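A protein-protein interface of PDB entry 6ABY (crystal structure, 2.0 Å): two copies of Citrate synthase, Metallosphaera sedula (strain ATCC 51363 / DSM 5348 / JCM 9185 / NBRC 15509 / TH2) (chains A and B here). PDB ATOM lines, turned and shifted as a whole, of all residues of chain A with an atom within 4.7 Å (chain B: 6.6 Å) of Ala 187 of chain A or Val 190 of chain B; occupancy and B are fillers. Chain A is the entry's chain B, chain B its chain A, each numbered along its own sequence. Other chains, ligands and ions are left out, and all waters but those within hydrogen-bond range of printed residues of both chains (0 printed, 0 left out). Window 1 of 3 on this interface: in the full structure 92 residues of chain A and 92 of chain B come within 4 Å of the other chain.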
ATOM      1  N   ALA A 183      -4.888   9.515  14.559  1.00  0.00           N
ATOM      2  CA  ALA A 183      -5.673  10.743  14.846  1.00  0.00           C
ATOM      3  C   ALA A 183      -6.222  10.727  16.288  1.00  0.00           C
ATOM      4  O   ALA A 183      -6.138  11.781  16.959  1.00  0.00           O
ATOM      5  CB  ALA A 183      -6.781  10.932  13.840  1.00  0.00           C
ATOM      6  N   SER A 184      -6.779   9.607  16.763  1.00  0.00           N
ATOM      7  CA  SER A 184      -7.383   9.513  18.127  1.00  0.00           C
ATOM      8  C   SER A 184      -6.301   9.695  19.196  1.00  0.00           C
ATOM      9  O   SER A 184      -6.539  10.438  20.162  1.00  0.00           O
ATOM     10  CB  SER A 184      -8.226   8.246  18.313  1.00  0.00           C
ATOM     11  OG  SER A 184      -7.448   7.031  18.207  1.00  0.00           O
ATOM     12  N   THR A 185      -5.145   9.057  19.058  1.00  0.00           N
ATOM     13  CA  THR A 185      -4.047   9.215  20.042  1.00  0.00           C
ATOM     14  C   THR A 185      -3.621  10.679  20.026  1.00  0.00           C
ATOM     15  O   THR A 185      -3.424  11.282  21.122  1.00  0.00           O
ATOM     16  CB  THR A 185      -2.873   8.256  19.799  1.00  0.00           C
ATOM     17  OG1 THR A 185      -3.386   6.915  19.799  1.00  0.00           O
ATOM     18  CG2 THR A 185      -1.823   8.429  20.871  1.00  0.00           C
ATOM     19  N   MET A 186      -3.553  11.255  18.839  1.00  0.00           N
ATOM     20  CA  MET A 186      -3.106  12.672  18.690  1.00  0.00           C
ATOM     21  C   MET A 186      -4.120  13.616  19.381  1.00  0.00           C
ATOM     22  O   MET A 186      -3.664  14.512  20.129  1.00  0.00           O
ATOM     23  CB  MET A 186      -2.880  13.025  17.218  1.00  0.00           C
ATOM     24  CG  MET A 186      -2.433  14.454  16.994  1.00  0.00           C
ATOM     25  SD  MET A 186      -0.896  14.807  17.866  1.00  0.00           S
ATOM     26  CE  MET A 186      -0.515  16.374  17.075  1.00  0.00           C
ATOM     27  N   ALA A 187      -5.427  13.411  19.206  1.00  0.00           N
ATOM     28  CA  ALA A 187      -6.496  14.221  19.853  1.00  0.00           C
ATOM     29  C   ALA A 187      -6.325  14.155  21.372  1.00  0.00           C
ATOM     30  O   ALA A 187      -6.396  15.234  22.029  1.00  0.00           O
ATOM     31  CB  ALA A 187      -7.887  13.776  19.452  1.00  0.00           C
ATOM     32  N   CYS A 188      -6.112  12.957  21.914  1.00  0.00           N
ATOM     33  CA  CYS A 188      -5.865  12.748  23.367  1.00  0.00           C
ATOM     34  C   CYS A 188      -4.667  13.586  23.825  1.00  0.00           C
ATOM     35  O   CYS A 188      -4.740  14.159  24.928  1.00  0.00           O
ATOM     36  CB  CYS A 188      -5.571  11.293  23.726  1.00  0.00           C
ATOM     37  SG  CYS A 188      -6.982  10.191  23.470  1.00  0.00           S
ATOM     38  N   LEU A 189      -3.559  13.535  23.078  1.00  0.00           N
ATOM     39  CA  LEU A 189      -2.285  14.185  23.467  1.00  0.00           C
ATOM     40  C   LEU A 189      -2.435  15.718  23.395  1.00  0.00           C
ATOM     41  O   LEU A 189      -1.911  16.401  24.285  1.00  0.00           O
ATOM     42  CB  LEU A 189      -1.156  13.654  22.592  1.00  0.00           C
ATOM     43  CG  LEU A 189      -0.728  12.213  22.867  1.00  0.00           C
ATOM     44  CD1 LEU A 189       0.181  11.706  21.803  1.00  0.00           C
ATOM     45  CD2 LEU A 189      -0.068  12.049  24.199  1.00  0.00           C
ATOM     46  N   VAL A 190      -3.124  16.238  22.377  1.00  0.00           N
ATOM     47  CA  VAL A 190      -3.326  17.708  22.205  1.00  0.00           C
ATOM     48  C   VAL A 190      -4.017  18.225  23.469  1.00  0.00           C
ATOM     49  O   VAL A 190      -3.516  19.164  24.083  1.00  0.00           O
ATOM     50  CB  VAL A 190      -4.128  18.041  20.943  1.00  0.00           C
ATOM     51  CG1 VAL A 190      -4.554  19.497  20.913  1.00  0.00           C
ATOM     52  CG2 VAL A 190      -3.361  17.698  19.683  1.00  0.00           C
ATOM     53  N   VAL A 191      -5.102  17.564  23.860  1.00  0.00           N
ATOM     54  CA  VAL A 191      -5.883  17.899  25.066  1.00  0.00           C
ATOM     55  C   VAL A 191      -5.024  17.741  26.329  1.00  0.00           C
ATOM     56  O   VAL A 191      -5.053  18.659  27.176  1.00  0.00           O
ATOM     57  CB  VAL A 191      -7.191  17.092  25.100  1.00  0.00           C
ATOM     58  CG1 VAL A 191      -7.876  17.234  26.426  1.00  0.00           C
ATOM     59  CG2 VAL A 191      -8.117  17.463  23.967  1.00  0.00           C
ATOM     60  N   ALA A 204     -11.905  13.441  23.842  1.00  0.00           N
ATOM     61  CA  ALA A 204     -11.371  13.890  22.550  1.00  0.00           C
ATOM     62  C   ALA A 204     -10.954  12.663  21.708  1.00  0.00           C
ATOM     63  O   ALA A 204     -11.221  12.657  20.515  1.00  0.00           O
ATOM     64  CB  ALA A 204     -10.233  14.830  22.793  1.00  0.00           C
ATOM     65  N   GLY A 205     -10.306  11.653  22.289  1.00  0.00           N
ATOM     66  CA  GLY A 205     -10.015  10.394  21.570  1.00  0.00           C
ATOM     67  C   GLY A 205     -11.257   9.770  20.935  1.00  0.00           C
ATOM     68  O   GLY A 205     -11.220   9.348  19.723  1.00  0.00           O
ATOM     69  N   ALA A 208     -12.581  11.727  17.931  1.00  0.00           N
ATOM     70  CA  ALA A 208     -11.757  11.478  16.731  1.00  0.00           C
ATOM     71  C   ALA A 208     -12.043  10.068  16.220  1.00  0.00           C
ATOM     72  O   ALA A 208     -12.151   9.906  15.000  1.00  0.00           O
ATOM     73  CB  ALA A 208     -10.276  11.665  16.991  1.00  0.00           C
ATOM     74  N   THR B 185      -7.723  24.918  18.944  1.00  0.00           N
ATOM     75  CA  THR B 185      -8.064  24.854  17.490  1.00  0.00           C
ATOM     76  C   THR B 185      -7.519  23.541  16.921  1.00  0.00           C
ATOM     77  O   THR B 185      -8.205  22.882  16.119  1.00  0.00           O
ATOM     78  CB  THR B 185      -7.527  26.063  16.721  1.00  0.00           C
ATOM     79  OG1 THR B 185      -7.871  27.249  17.442  1.00  0.00           O
ATOM     80  CG2 THR B 185      -8.088  26.126  15.312  1.00  0.00           C
ATOM     81  N   MET B 186      -6.328  23.163  17.348  1.00  0.00           N
ATOM     82  CA  MET B 186      -5.672  21.932  16.861  1.00  0.00           C
ATOM     83  C   MET B 186      -6.546  20.729  17.252  1.00  0.00           C
ATOM     84  O   MET B 186      -6.845  19.907  16.356  1.00  0.00           O
ATOM     85  CB  MET B 186      -4.235  21.850  17.380  1.00  0.00           C
ATOM     86  CG  MET B 186      -3.474  20.633  16.906  1.00  0.00           C
ATOM     87  SD  MET B 186      -3.386  20.567  15.115  1.00  0.00           S
ATOM     88  CE  MET B 186      -2.176  19.241  15.050  1.00  0.00           C
ATOM     89  N   ALA B 187      -7.043  20.653  18.496  1.00  0.00           N
ATOM     90  CA  ALA B 187      -7.958  19.566  18.937  1.00  0.00           C
ATOM     91  C   ALA B 187      -9.212  19.474  18.054  1.00  0.00           C
ATOM     92  O   ALA B 187      -9.565  18.341  17.672  1.00  0.00           O
ATOM     93  CB  ALA B 187      -8.324  19.706  20.404  1.00  0.00           C
ATOM     94  N   CYS B 188      -9.902  20.585  17.764  1.00  0.00           N
ATOM     95  CA  CYS B 188     -11.042  20.602  16.824  1.00  0.00           C
ATOM     96  C   CYS B 188     -10.623  20.040  15.445  1.00  0.00           C
ATOM     97  O   CYS B 188     -11.398  19.309  14.858  1.00  0.00           O
ATOM     98  CB  CYS B 188     -11.594  22.007  16.614  1.00  0.00           C
ATOM     99  SG  CYS B 188     -12.188  22.770  18.142  1.00  0.00           S
ATOM    100  N   LEU B 189      -9.468  20.440  14.927  1.00  0.00           N
ATOM    101  CA  LEU B 189      -9.061  20.093  13.541  1.00  0.00           C
ATOM    102  C   LEU B 189      -8.715  18.595  13.502  1.00  0.00           C
ATOM    103  O   LEU B 189      -9.100  17.926  12.535  1.00  0.00           O
ATOM    104  CB  LEU B 189      -7.871  20.973  13.174  1.00  0.00           C
ATOM    105  CG  LEU B 189      -8.203  22.432  12.864  1.00  0.00           C
ATOM    106  CD1 LEU B 189      -6.921  23.186  12.574  1.00  0.00           C
ATOM    107  CD2 LEU B 189      -9.167  22.529  11.680  1.00  0.00           C
ATOM    108  N   VAL B 190      -7.991  18.091  14.515  1.00  0.00           N
ATOM    109  CA  VAL B 190      -7.594  16.647  14.532  1.00  0.00           C
ATOM    110  C   VAL B 190      -8.877  15.824  14.451  1.00  0.00           C
ATOM    111  O   VAL B 190      -8.989  14.916  13.600  1.00  0.00           O
ATOM    112  CB  VAL B 190      -6.748  16.288  15.758  1.00  0.00           C
ATOM    113  CG1 VAL B 190      -6.554  14.777  15.851  1.00  0.00           C
ATOM    114  CG2 VAL B 190      -5.415  17.019  15.760  1.00  0.00           C
ATOM    115  N   VAL B 191      -9.860  16.157  15.279  1.00  0.00           N
ATOM    116  CA  VAL B 191     -11.173  15.451  15.267  1.00  0.00           C
ATOM    117  C   VAL B 191     -11.907  15.668  13.925  1.00  0.00           C
ATOM    118  O   VAL B 191     -12.424  14.705  13.371  1.00  0.00           O
ATOM    119  CB  VAL B 191     -11.994  15.900  16.487  1.00  0.00           C
ATOM    120  CG1 VAL B 191     -13.421  15.447  16.368  1.00  0.00           C
ATOM    121  CG2 VAL B 191     -11.328  15.416  17.776  1.00  0.00           C
ATOM    122  N   ALA B 192     -11.982  16.880  13.384  1.00  0.00           N
ATOM    123  CA  ALA B 192     -12.657  17.114  12.077  1.00  0.00           C
ATOM    124  C   ALA B 192     -11.979  16.291  10.973  1.00  0.00           C
ATOM    125  O   ALA B 192     -12.686  15.874  10.076  1.00  0.00           O
ATOM    126  CB  ALA B 192     -12.651  18.569  11.702  1.00  0.00           C
ATOM    127  N   SER B 193     -10.662  16.135  11.026  1.00  0.00           N
ATOM    128  CA  SER B 193      -9.835  15.523   9.950  1.00  0.00           C
ATOM    129  C   SER B 193     -10.238  14.070   9.707  1.00  0.00           C
ATOM    130  O   SER B 193     -10.009  13.571   8.565  1.00  0.00           O
ATOM    131  CB  SER B 193      -8.378  15.648  10.232  1.00  0.00           C
ATOM    132  OG  SER B 193      -7.944  14.721  11.196  1.00  0.00           O
ATOM    133  N   THR B 194     -10.881  13.434  10.683  1.00  0.00           N
ATOM    134  CA  THR B 194     -11.376  12.036  10.570  1.00  0.00           C
ATOM    135  C   THR B 194     -12.777  11.998   9.959  1.00  0.00           C
ATOM    136  O   THR B 194     -13.269  10.858   9.731  1.00  0.00           O
ATOM    137  CB  THR B 194     -11.452  11.332  11.939  1.00  0.00           C
ATOM    138  OG1 THR B 194     -12.535  11.926  12.670  1.00  0.00           O
ATOM    139  CG2 THR B 194     -10.143  11.374  12.681  1.00  0.00           C
ATOM    140  N   LEU B 195     -13.367  13.175   9.703  1.00  0.00           N
ATOM    141  CA  LEU B 195     -14.757  13.425   9.218  1.00  0.00           C
ATOM    142  C   LEU B 195     -15.731  13.079  10.328  1.00  0.00           C
ATOM    143  O   LEU B 195     -16.876  12.769  10.033  1.00  0.00           O
ATOM    144  CB  LEU B 195     -15.068  12.660   7.921  1.00  0.00           C
ATOM    145  CG  LEU B 195     -14.158  13.027   6.744  1.00  0.00           C
ATOM    146  CD1 LEU B 195     -14.553  12.268   5.475  1.00  0.00           C
ATOM    147  CD2 LEU B 195     -14.194  14.530   6.488  1.00  0.00           C
ATOM    148  N   SER B 201     -15.972  17.875  17.249  1.00  0.00           N
ATOM    149  CA  SER B 201     -14.845  18.820  17.117  1.00  0.00           C
ATOM    150  C   SER B 201     -14.871  19.850  18.255  1.00  0.00           C
ATOM    151  O   SER B 201     -13.820  20.028  18.903  1.00  0.00           O
ATOM    152  CB  SER B 201     -14.804  19.518  15.783  1.00  0.00           C
ATOM    153  OG  SER B 201     -14.674  18.583  14.736  1.00  0.00           O
ATOM    154  N   ALA B 204     -14.045  18.462  21.633  1.00  0.00           N
ATOM    155  CA  ALA B 204     -12.580  18.329  21.757  1.00  0.00           C
ATOM    156  C   ALA B 204     -11.951  19.701  22.064  1.00  0.00           C
ATOM    157  O   ALA B 204     -10.999  19.760  22.855  1.00  0.00           O
ATOM    158  CB  ALA B 204     -11.960  17.704  20.531  1.00  0.00           C
ATOM    159  N   LEU B 349      -6.474  13.874   6.647  1.00  0.00           N
ATOM    160  CA  LEU B 349      -6.416  13.129   7.928  1.00  0.00           C
ATOM    161  C   LEU B 349      -5.142  13.539   8.655  1.00  0.00           C
ATOM    162  O   LEU B 349      -4.068  13.501   8.058  1.00  0.00           O
ATOM    163  CB  LEU B 349      -6.454  11.623   7.636  1.00  0.00           C
ATOM    164  CG  LEU B 349      -6.357  10.713   8.863  1.00  0.00           C
ATOM    165  CD1 LEU B 349      -7.531  10.934   9.805  1.00  0.00           C
ATOM    166  CD2 LEU B 349      -6.270   9.242   8.437  1.00  0.00           C
ATOM    167  N   ILE B 350      -5.249  13.952   9.912  1.00  0.00           N
ATOM    168  CA  ILE B 350      -4.054  14.330  10.698  1.00  0.00           C
ATOM    169  C   ILE B 350      -3.572  13.057  11.388  1.00  0.00           C
ATOM    170  O   ILE B 350      -4.306  12.528  12.279  1.00  0.00           O
ATOM    171  CB  ILE B 350      -4.356  15.510  11.641  1.00  0.00           C
ATOM    172  CG1 ILE B 350      -4.794  16.738  10.832  1.00  0.00           C
ATOM    173  CG2 ILE B 350      -3.148  15.774  12.537  1.00  0.00           C
ATOM    174  CD1 ILE B 350      -5.411  17.880  11.615  1.00  0.00           C
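Hydrophobic or aromatic side chains of chain A within 4 Å of the printed part of chain B: Ala 183, Met 186, Ala 187, Val 190, Val 191 and Ala 208.
Among the printed residues, 10 pairs touch across the chains.
Among the printed residues, no Asp or Glu carboxylate lies within 4 Å of a Lys or Arg side-chain nitrogen of the other chain.
Of the printed residues of chain B, Met 186 of chain A touches Met 186.
Ala 187 of chain A touches just one residue of chain B: Val 190 (3.8 Å).
Of the printed residues of chain B, Val 191 of chain A touches Ala 204 (3.8 Å).
Printed residues of chain A within 4 Å of Thr 194 of chain B: Ala 183 (3.6 Å) and Ala 208 (3.1 Å).
The nearest residue of chain A that does not touch Val 190 of chain B is Met 186 of chain A (4.1 Å).
Met 186 of chain B touches its own counterpart, Met 186 of chain A.
Ala 187 of chain A touches Val 190 of chain B, and with the chains exchanged Val 190 of chain A touches Ala 187 of chain B.
Val 191 of chain A touches Ala 204 of chain B, and with the chains exchanged Ala 204 of chain A touches Val 191 of chain B.
8 positions are printed for both chains.
Of the 10 pairs that touch across the chains among the printed residues, 5 have their exchanged pair printed and touching as well.
N of Ile 350 of chain B is in hydrogen-bond range of OG of Ser 193 of chain B (3.1 Å).
O of Val 190 of chain B sits at hydrogen-bond distance from OG of Ser 193 of chain B (2.6 Å).
O of Val 191 of chain B is in hydrogen-bond range of OG1 of Thr 194 of chain B, 2.9 Å away.
The side-chain hydroxyl of Thr 194 of chain B lies within hydrogen-bond range of the backbone carbonyl oxygen of Ala 208 of chain A, at 3.1 Å.
Val 190 of chain B touches Ala 183 of chain A.
CB of Ala 183 of chain A touches CG2 of Thr 194 of chain B, 3.6 Å away.
CB of Ala 183 of chain A touches O of Ile 350 of chain B (3.3 Å).
Met 186 of chain B touches Met 186 of chain A (CE to CE, 3.9 Å).
CG1 of Val 190 of chain B touches N of Ala 187 of chain A, at 3.8 Å.
CG1 of Val 190 of chain A touches N of Ala 187 of chain B, 3.7 Å away.
Val 191 of chain A touches Ala 204 of chain B.
Val 191 of chain B touches Ala 204 of chain A (CG2 to O, 3.9 Å).
Val 191 of chain B touches Ala 208 of chain A.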
